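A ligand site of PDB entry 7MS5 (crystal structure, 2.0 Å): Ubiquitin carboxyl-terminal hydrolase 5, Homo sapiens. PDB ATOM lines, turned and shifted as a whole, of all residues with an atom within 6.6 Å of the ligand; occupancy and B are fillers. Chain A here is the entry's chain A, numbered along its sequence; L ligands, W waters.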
ATOM      1  N   ARG A   5     -36.874  -6.841   1.646  1.00  0.00           N
ATOM      2  CA  ARG A   5     -37.451  -7.841   0.712  1.00  0.00           C
ATOM      3  C   ARG A   5     -38.963  -7.714   0.706  1.00  0.00           C
ATOM      4  O   ARG A   5     -39.598  -7.925   1.753  1.00  0.00           O
ATOM      5  CB  ARG A   5     -36.932  -9.243   1.024  1.00  0.00           C
ATOM      6  CG  ARG A   5     -35.445  -9.375   0.721  1.00  0.00           C
ATOM      7  CD  ARG A   5     -34.883 -10.606   1.345  1.00  0.00           C
ATOM      8  NE  ARG A   5     -33.440 -10.672   1.241  1.00  0.00           N
ATOM      9  CZ  ARG A   5     -32.731 -11.731   1.573  1.00  0.00           C
ATOM     10  NH1 ARG A   5     -33.349 -12.825   2.032  1.00  0.00           N
ATOM     11  NH2 ARG A   5     -31.410 -11.713   1.460  1.00  0.00           N
ATOM     12  N   ASN A  38     -24.574 -24.051  -3.312  1.00  0.00           N
ATOM     13  CA  ASN A  38     -25.290 -23.053  -4.154  1.00  0.00           C
ATOM     14  C   ASN A  38     -26.433 -23.744  -4.918  1.00  0.00           C
ATOM     15  O   ASN A  38     -26.524 -23.579  -6.175  1.00  0.00           O
ATOM     16  CB  ASN A  38     -24.306 -22.397  -5.107  1.00  0.00           C
ATOM     17  CG  ASN A  38     -24.893 -21.207  -5.811  1.00  0.00           C
ATOM     18  OD1 ASN A  38     -25.877 -20.628  -5.352  1.00  0.00           O
ATOM     19  ND2 ASN A  38     -24.307 -20.851  -6.943  1.00  0.00           N
ATOM     20  N   TRP A  40     -30.650 -24.449  -5.401  1.00  0.00           N
ATOM     21  CA  TRP A  40     -31.940 -23.758  -5.279  1.00  0.00           C
ATOM     22  C   TRP A  40     -33.074 -24.751  -5.502  1.00  0.00           C
ATOM     23  O   TRP A  40     -33.088 -25.447  -6.554  1.00  0.00           O
ATOM     24  CB  TRP A  40     -31.992 -22.567  -6.237  1.00  0.00           C
ATOM     25  CG  TRP A  40     -30.990 -21.515  -5.863  1.00  0.00           C
ATOM     26  CD1 TRP A  40     -29.654 -21.518  -6.149  1.00  0.00           C
ATOM     27  CD2 TRP A  40     -31.246 -20.312  -5.132  1.00  0.00           C
ATOM     28  NE1 TRP A  40     -29.064 -20.393  -5.642  1.00  0.00           N
ATOM     29  CE2 TRP A  40     -30.012 -19.636  -5.020  1.00  0.00           C
ATOM     30  CE3 TRP A  40     -32.400 -19.724  -4.620  1.00  0.00           C
ATOM     31  CZ2 TRP A  40     -29.910 -18.400  -4.382  1.00  0.00           C
ATOM     32  CZ3 TRP A  40     -32.291 -18.512  -3.964  1.00  0.00           C
ATOM     33  CH2 TRP A  40     -31.063 -17.865  -3.861  1.00  0.00           C
ATOM     34  N   LEU A  49     -31.422 -27.456  -8.217  1.00  0.00           N
ATOM     35  CA  LEU A  49     -30.548 -27.070  -9.359  1.00  0.00           C
ATOM     36  C   LEU A  49     -29.614 -25.939  -8.926  1.00  0.00           C
ATOM     37  O   LEU A  49     -30.002 -25.121  -8.064  1.00  0.00           O
ATOM     38  CB  LEU A  49     -31.426 -26.657 -10.533  1.00  0.00           C
ATOM     39  CG  LEU A  49     -32.287 -27.760 -11.144  1.00  0.00           C
ATOM     40  CD1 LEU A  49     -33.334 -27.163 -12.062  1.00  0.00           C
ATOM     41  CD2 LEU A  49     -31.445 -28.771 -11.917  1.00  0.00           C
ATOM     42  N   CYS A  50     -28.459 -25.834  -9.542  1.00  0.00           N
ATOM     43  CA  CYS A  50     -27.412 -24.885  -9.101  1.00  0.00           C
ATOM     44  C   CYS A  50     -27.732 -23.442  -9.532  1.00  0.00           C
ATOM     45  O   CYS A  50     -28.439 -23.207 -10.546  1.00  0.00           O
ATOM     46  CB  CYS A  50     -26.040 -25.340  -9.557  1.00  0.00           C
ATOM     47  SG  CYS A  50     -25.872 -25.519 -11.349  1.00  0.00           S
ATOM     48  N   GLY A  51     -27.185 -22.515  -8.767  1.00  0.00           N
ATOM     49  CA  GLY A  51     -27.327 -21.071  -8.975  1.00  0.00           C
ATOM     50  C   GLY A  51     -26.583 -20.626 -10.209  1.00  0.00           C
ATOM     51  O   GLY A  51     -25.776 -21.402 -10.791  1.00  0.00           O
ATOM     52  N   ARG A  52     -26.858 -19.401 -10.613  1.00  0.00           N
ATOM     53  CA  ARG A  52     -26.336 -18.849 -11.865  1.00  0.00           C
ATOM     54  C   ARG A  52     -24.849 -18.490 -11.751  1.00  0.00           C
ATOM     55  O   ARG A  52     -24.329 -18.234 -10.633  1.00  0.00           O
ATOM     56  CB  ARG A  52     -27.226 -17.678 -12.254  1.00  0.00           C
ATOM     57  CG  ARG A  52     -27.022 -16.415 -11.453  1.00  0.00           C
ATOM     58  CD  ARG A  52     -27.617 -15.285 -12.306  1.00  0.00           C
ATOM     59  NE  ARG A  52     -28.977 -15.132 -12.001  1.00  0.00           N
ATOM     60  CZ  ARG A  52     -29.952 -14.754 -12.819  1.00  0.00           C
ATOM     61  NH1 ARG A  52     -31.173 -14.694 -12.309  1.00  0.00           N
ATOM     62  NH2 ARG A  52     -29.767 -14.492 -14.121  1.00  0.00           N
ATOM     63  N   ARG A  53     -24.200 -18.406 -12.902  1.00  0.00           N
ATOM     64  CA  ARG A  53     -22.876 -17.778 -13.094  1.00  0.00           C
ATOM     65  C   ARG A  53     -23.079 -16.269 -13.166  1.00  0.00           C
ATOM     66  O   ARG A  53     -23.731 -15.794 -14.111  1.00  0.00           O
ATOM     67  CB  ARG A  53     -22.221 -18.318 -14.370  1.00  0.00           C
ATOM     68  CG  ARG A  53     -20.724 -18.072 -14.450  1.00  0.00           C
ATOM     69  CD  ARG A  53     -19.955 -18.924 -13.447  1.00  0.00           C
ATOM     70  NE  ARG A  53     -20.162 -20.334 -13.737  1.00  0.00           N
ATOM     71  CZ  ARG A  53     -19.423 -21.057 -14.577  1.00  0.00           C
ATOM     72  NH1 ARG A  53     -18.374 -20.526 -15.175  1.00  0.00           N
ATOM     73  NH2 ARG A  53     -19.733 -22.323 -14.805  1.00  0.00           N
ATOM     74  N   TYR A  54     -22.623 -15.556 -12.152  1.00  0.00           N
ATOM     75  CA  TYR A  54     -22.594 -14.075 -12.131  1.00  0.00           C
ATOM     76  C   TYR A  54     -21.538 -13.570 -13.147  1.00  0.00           C
ATOM     77  O   TYR A  54     -20.669 -14.347 -13.623  1.00  0.00           O
ATOM     78  CB  TYR A  54     -22.359 -13.572 -10.706  1.00  0.00           C
ATOM     79  CG  TYR A  54     -23.478 -13.873  -9.750  1.00  0.00           C
ATOM     80  CD1 TYR A  54     -24.735 -13.286  -9.882  1.00  0.00           C
ATOM     81  CD2 TYR A  54     -23.278 -14.717  -8.675  1.00  0.00           C
ATOM     82  CE1 TYR A  54     -25.751 -13.567  -9.000  1.00  0.00           C
ATOM     83  CE2 TYR A  54     -24.282 -14.971  -7.760  1.00  0.00           C
ATOM     84  CZ  TYR A  54     -25.538 -14.413  -7.927  1.00  0.00           C
ATOM     85  OH  TYR A  54     -26.527 -14.676  -7.008  1.00  0.00           O
ATOM     86  N   ASP A  56     -19.117 -11.758 -12.808  1.00  0.00           N
ATOM     87  CA  ASP A  56     -17.727 -11.803 -12.286  1.00  0.00           C
ATOM     88  C   ASP A  56     -17.144 -13.208 -12.471  1.00  0.00           C
ATOM     89  O   ASP A  56     -15.984 -13.374 -12.185  1.00  0.00           O
ATOM     90  CB  ASP A  56     -17.652 -11.315 -10.841  1.00  0.00           C
ATOM     91  CG  ASP A  56     -18.268 -12.243  -9.802  1.00  0.00           C
ATOM     92  OD1 ASP A  56     -19.022 -13.176 -10.200  1.00  0.00           O
ATOM     93  OD2 ASP A  56     -18.066 -11.974  -8.610  1.00  0.00           O
ATOM     94  N   SER A  58     -18.069 -15.867 -10.681  1.00  0.00           N
ATOM     95  CA  SER A  58     -18.480 -16.634  -9.473  1.00  0.00           C
ATOM     96  C   SER A  58     -19.852 -17.284  -9.716  1.00  0.00           C
ATOM     97  O   SER A  58     -20.557 -16.876 -10.682  1.00  0.00           O
ATOM     98  CB  SER A  58     -18.519 -15.789  -8.219  1.00  0.00           C
ATOM     99  OG  SER A  58     -19.710 -14.991  -8.151  1.00  0.00           O
ATOM    100  N   ASN A  62     -25.830 -22.419 -13.827  1.00  0.00           N
ATOM    101  CA  ASN A  62     -27.072 -21.811 -14.406  1.00  0.00           C
ATOM    102  C   ASN A  62     -28.236 -22.809 -14.475  1.00  0.00           C
ATOM    103  O   ASN A  62     -29.224 -22.497 -15.177  1.00  0.00           O
ATOM    104  CB  ASN A  62     -26.812 -21.272 -15.816  1.00  0.00           C
ATOM    105  CG  ASN A  62     -25.797 -20.155 -15.802  1.00  0.00           C
ATOM    106  OD1 ASN A  62     -25.919 -19.226 -15.010  1.00  0.00           O
ATOM    107  ND2 ASN A  62     -24.757 -20.301 -16.616  1.00  0.00           N
ATOM    108  N   HIS A  63     -28.187 -23.935 -13.785  1.00  0.00           N
ATOM    109  CA  HIS A  63     -29.190 -25.014 -13.989  1.00  0.00           C
ATOM    110  C   HIS A  63     -30.578 -24.558 -13.477  1.00  0.00           C
ATOM    111  O   HIS A  63     -31.584 -24.798 -14.181  1.00  0.00           O
ATOM    112  CB  HIS A  63     -28.647 -26.361 -13.493  1.00  0.00           C
ATOM    113  CG  HIS A  63     -27.625 -26.940 -14.407  1.00  0.00           C
ATOM    114  ND1 HIS A  63     -26.456 -27.521 -13.939  1.00  0.00           N
ATOM    115  CD2 HIS A  63     -27.564 -26.973 -15.761  1.00  0.00           C
ATOM    116  CE1 HIS A  63     -25.716 -27.888 -14.972  1.00  0.00           C
ATOM    117  NE2 HIS A  63     -26.383 -27.599 -16.101  1.00  0.00           N
ATOM    118  N   ALA A  64     -30.645 -23.834 -12.354  1.00  0.00           N
ATOM    119  CA  ALA A  64     -31.921 -23.356 -11.788  1.00  0.00           C
ATOM    120  C   ALA A  64     -32.508 -22.283 -12.727  1.00  0.00           C
ATOM    121  O   ALA A  64     -33.727 -22.378 -12.994  1.00  0.00           O
ATOM    122  CB  ALA A  64     -31.752 -22.859 -10.360  1.00  0.00           C
ATOM    123  N   VAL A  65     -31.674 -21.397 -13.286  1.00  0.00           N
ATOM    124  CA  VAL A  65     -32.204 -20.305 -14.178  1.00  0.00           C
ATOM    125  C   VAL A  65     -32.667 -20.921 -15.500  1.00  0.00           C
ATOM    126  O   VAL A  65     -33.695 -20.479 -15.966  1.00  0.00           O
ATOM    127  CB  VAL A  65     -31.249 -19.124 -14.427  1.00  0.00           C
ATOM    128  CG1 VAL A  65     -31.149 -18.243 -13.198  1.00  0.00           C
ATOM    129  CG2 VAL A  65     -29.879 -19.537 -14.914  1.00  0.00           C
ATOM    130  N   ALA A  76     -37.788 -19.825  -5.963  1.00  0.00           N
ATOM    131  CA  ALA A  76     -36.809 -20.843  -5.513  1.00  0.00           C
ATOM    132  C   ALA A  76     -36.243 -20.426  -4.156  1.00  0.00           C
ATOM    133  O   ALA A  76     -36.048 -19.240  -3.954  1.00  0.00           O
ATOM    134  CB  ALA A  76     -35.732 -20.984  -6.546  1.00  0.00           C
ATOM    135  N   TYR A  90     -35.757 -16.333  -3.946  1.00  0.00           N
ATOM    136  CA  TYR A  90     -35.576 -15.528  -5.187  1.00  0.00           C
ATOM    137  C   TYR A  90     -36.785 -15.713  -6.092  1.00  0.00           C
ATOM    138  O   TYR A  90     -37.316 -16.830  -6.175  1.00  0.00           O
ATOM    139  CB  TYR A  90     -34.305 -15.895  -5.934  1.00  0.00           C
ATOM    140  CG  TYR A  90     -33.924 -14.870  -6.972  1.00  0.00           C
ATOM    141  CD1 TYR A  90     -33.405 -13.660  -6.570  1.00  0.00           C
ATOM    142  CD2 TYR A  90     -34.041 -15.108  -8.353  1.00  0.00           C
ATOM    143  CE1 TYR A  90     -33.037 -12.683  -7.478  1.00  0.00           C
ATOM    144  CE2 TYR A  90     -33.683 -14.129  -9.272  1.00  0.00           C
ATOM    145  CZ  TYR A  90     -33.190 -12.910  -8.833  1.00  0.00           C
ATOM    146  OH  TYR A  90     -32.800 -11.903  -9.669  1.00  0.00           O
ATOM    147  N   TYR A  92     -37.496 -15.267 -10.030  1.00  0.00           N
ATOM    148  CA  TYR A  92     -36.890 -15.083 -11.366  1.00  0.00           C
ATOM    149  C   TYR A  92     -37.695 -14.038 -12.147  1.00  0.00           C
ATOM    150  O   TYR A  92     -37.107 -13.260 -12.867  1.00  0.00           O
ATOM    151  CB  TYR A  92     -36.843 -16.411 -12.120  1.00  0.00           C
ATOM    152  CG  TYR A  92     -35.876 -17.396 -11.527  1.00  0.00           C
ATOM    153  CD1 TYR A  92     -34.514 -17.214 -11.668  1.00  0.00           C
ATOM    154  CD2 TYR A  92     -36.316 -18.530 -10.851  1.00  0.00           C
ATOM    155  CE1 TYR A  92     -33.611 -18.122 -11.148  1.00  0.00           C
ATOM    156  CE2 TYR A  92     -35.421 -19.460 -10.348  1.00  0.00           C
ATOM    157  CZ  TYR A  92     -34.057 -19.255 -10.497  1.00  0.00           C
ATOM    158  OH  TYR A  92     -33.139 -20.147 -10.017  1.00  0.00           O
ATOM    159  N   ASP A  95     -37.257 -10.758 -10.538  1.00  0.00           N
ATOM    160  CA  ASP A  95     -35.776 -10.557 -10.563  1.00  0.00           C
ATOM    161  C   ASP A  95     -35.319  -9.857  -9.289  1.00  0.00           C
ATOM    162  O   ASP A  95     -34.721  -8.735  -9.363  1.00  0.00           O
ATOM    163  CB  ASP A  95     -35.355  -9.768 -11.805  1.00  0.00           C
ATOM    164  CG  ASP A  95     -33.880  -9.915 -12.119  1.00  0.00           C
ATOM    165  OD1 ASP A  95     -33.270 -10.875 -11.619  1.00  0.00           O
ATOM    166  OD2 ASP A  95     -33.346  -9.057 -12.872  1.00  0.00           O
ATOM    167  N   ASP A  96     -35.528 -10.503  -8.148  1.00  0.00           N
ATOM    168  CA  ASP A  96     -35.268  -9.960  -6.797  1.00  0.00           C
ATOM    169  C   ASP A  96     -35.355 -11.085  -5.757  1.00  0.00           C
ATOM    170  O   ASP A  96     -36.175 -11.966  -5.940  1.00  0.00           O
ATOM    171  CB  ASP A  96     -36.290  -8.869  -6.427  1.00  0.00           C
ATOM    172  CG  ASP A  96     -35.811  -7.453  -6.728  1.00  0.00           C
ATOM    173  OD1 ASP A  96     -34.641  -7.108  -6.332  1.00  0.00           O
ATOM    174  OD2 ASP A  96     -36.590  -6.696  -7.370  1.00  0.00           O
ATOM    175  N   MET A  97     -34.589 -10.968  -4.688  1.00  0.00           N
ATOM    176  CA  MET A  97     -34.857 -11.649  -3.402  1.00  0.00           C
ATOM    177  C   MET A  97     -36.208 -11.122  -2.904  1.00  0.00           C
ATOM    178  O   MET A  97     -36.451  -9.892  -3.026  1.00  0.00           O
ATOM    179  CB  MET A  97     -33.783 -11.340  -2.370  1.00  0.00           C
ATOM    180  CG  MET A  97     -32.393 -11.752  -2.807  1.00  0.00           C
ATOM    181  SD  MET A  97     -32.250 -13.515  -3.162  1.00  0.00           S
ATOM    182  CE  MET A  97     -32.656 -14.251  -1.583  1.00  0.00           C
HETATM  183  C1  LIG L   1     -20.596 -12.101  -6.044  1.00  0.00           C
HETATM  184  C2  LIG L   1     -20.103 -11.144  -5.186  1.00  0.00           C
HETATM  185  C3  LIG L   1     -20.939 -10.253  -4.585  1.00  0.00           C
HETATM  186  O1  LIG L   1     -28.930 -18.313  -9.007  1.00  0.00           O
HETATM  187  C4  LIG L   1     -26.421 -10.502  -6.868  1.00  0.00           C
HETATM  188  C5  LIG L   1     -22.821 -11.249  -5.660  1.00  0.00           C
HETATM  189  C6  LIG L   1     -21.967 -12.143  -6.278  1.00  0.00           C
HETATM  190  C7  LIG L   1     -24.325 -11.382  -5.835  1.00  0.00           C
HETATM  191  O2  LIG L   1     -29.177 -10.607  -4.245  1.00  0.00           O
HETATM  192  C8  LIG L   1     -25.070 -11.473  -4.499  1.00  0.00           C
HETATM  193  O3  LIG L   1     -29.096  -9.450  -6.440  1.00  0.00           O
HETATM  194  C9  LIG L   1     -26.556 -11.718  -4.740  1.00  0.00           C
HETATM  195  S1  LIG L   1     -28.746 -10.564  -5.608  1.00  0.00           S
HETATM  196  C10 LIG L   1     -29.327 -12.042  -6.370  1.00  0.00           C
HETATM  197  C11 LIG L   1     -29.595 -13.159  -5.599  1.00  0.00           C
HETATM  198  C12 LIG L   1     -29.953 -14.343  -6.205  1.00  0.00           C
HETATM  199  C13 LIG L   1     -30.091 -14.419  -7.596  1.00  0.00           C
HETATM  200  C14 LIG L   1     -30.602 -15.665  -8.246  1.00  0.00           C
HETATM  201  O4  LIG L   1     -30.802 -15.700  -9.457  1.00  0.00           O
HETATM  202  C15 LIG L   1     -30.825 -16.892  -7.400  1.00  0.00           C
HETATM  203  C16 LIG L   1     -31.215 -18.105  -8.243  1.00  0.00           C
HETATM  204  C17 LIG L   1     -30.125 -18.590  -9.154  1.00  0.00           C
HETATM  205  O5  LIG L   1     -30.564 -19.361 -10.088  1.00  0.00           O
HETATM  206  C18 LIG L   1     -29.839 -13.275  -8.358  1.00  0.00           C
HETATM  207  C19 LIG L   1     -29.445 -12.091  -7.756  1.00  0.00           C
HETATM  208  N1  LIG L   1     -27.118 -10.640  -5.576  1.00  0.00           N
HETATM  209  C20 LIG L   1     -24.931 -10.268  -6.662  1.00  0.00           C
HETATM  210  C21 LIG L   1     -22.297 -10.286  -4.800  1.00  0.00           C
HETATM  211  F1  LIG L   1     -20.403  -9.296  -3.796  1.00  0.00           F
HETATM  212  F2  LIG L   1     -18.773 -11.054  -4.973  1.00  0.00           F
HETATM  213  O   HOH W   1     -31.464  -9.209  -8.411  1.00  0.00           O
HETATM  214  O   HOH W   2     -22.973 -14.695  -4.278  1.00  0.00           O
HETATM  215  O   HOH W   3     -27.337 -17.341  -7.251  1.00  0.00           O
HETATM  216  O   HOH W   4     -16.513 -12.480  -6.678  1.00  0.00           O
HETATM  217  O   HOH W   5     -25.554 -15.056  -4.536  1.00  0.00           O
HETATM  218  O   HOH W   6     -29.146 -20.997 -11.952  1.00  0.00           O
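An oxygen (O4) of the ligand is in hydrogen-bond range of the guanidinium group (NH1) of Arg 52 (3.0 Å).
O5 of the ligand sits at hydrogen-bond distance from OH of Tyr 92.
The backbone NH (N) of Arg 52 sits at hydrogen-bond distance from an oxygen (O1) of the ligand (2.8 Å).
The backbone carbonyl oxygen (O) of Gly 51 is in hydrogen-bond range of the backbone NH (N) of Asn 62 (3.2 Å).
The backbone carbonyl oxygen (O) of Asn 38 sits at hydrogen-bond distance from the backbone NH (N) of Gly 51 (2.9 Å).
OD1 of Asn 38 lies within hydrogen-bond range of NE1 of Trp 40, 3.2 Å away.
The backbone NH of Ala 64 sits at hydrogen-bond distance from the backbone carbonyl oxygen of Cys 50 (2.9 Å).
The backbone NH (N) of Asp 96 sits close to the side-chain hydroxyl (OH) of Tyr 90.
N of Trp 40 sits at hydrogen-bond distance from O of Leu 49.
OD1 of Asp 56 is in hydrogen-bond range of OG of Ser 58 (2.8 Å).
N of Tyr 90 sits at hydrogen-bond distance from O of Ala 76, at 2.9 Å.
Residues that only touch the ligand: Gly 51 (3.2 Å), Tyr 90 (3.3 Å), Val 65 (3.4 Å), Trp 40 (3.5 Å), Tyr 54 (3.5 Å), Asp 56 (3.6 Å), Met 97 (3.6 Å), Ser 58 (3.7 Å) and Ala 64 (3.7 Å).
Of the 21 residues printed, 11 come within 4 Å of the ligand.
Water W3 bridges O1 of the ligand (2.6 Å) and OH of Tyr 54 (2.8 Å).
Water W1 lies within hydrogen-bond range of an oxygen (O3) of the ligand, the side-chain hydroxyl (OH) of Tyr 90 and the backbone carbonyl oxygen (O) of Asp 95.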
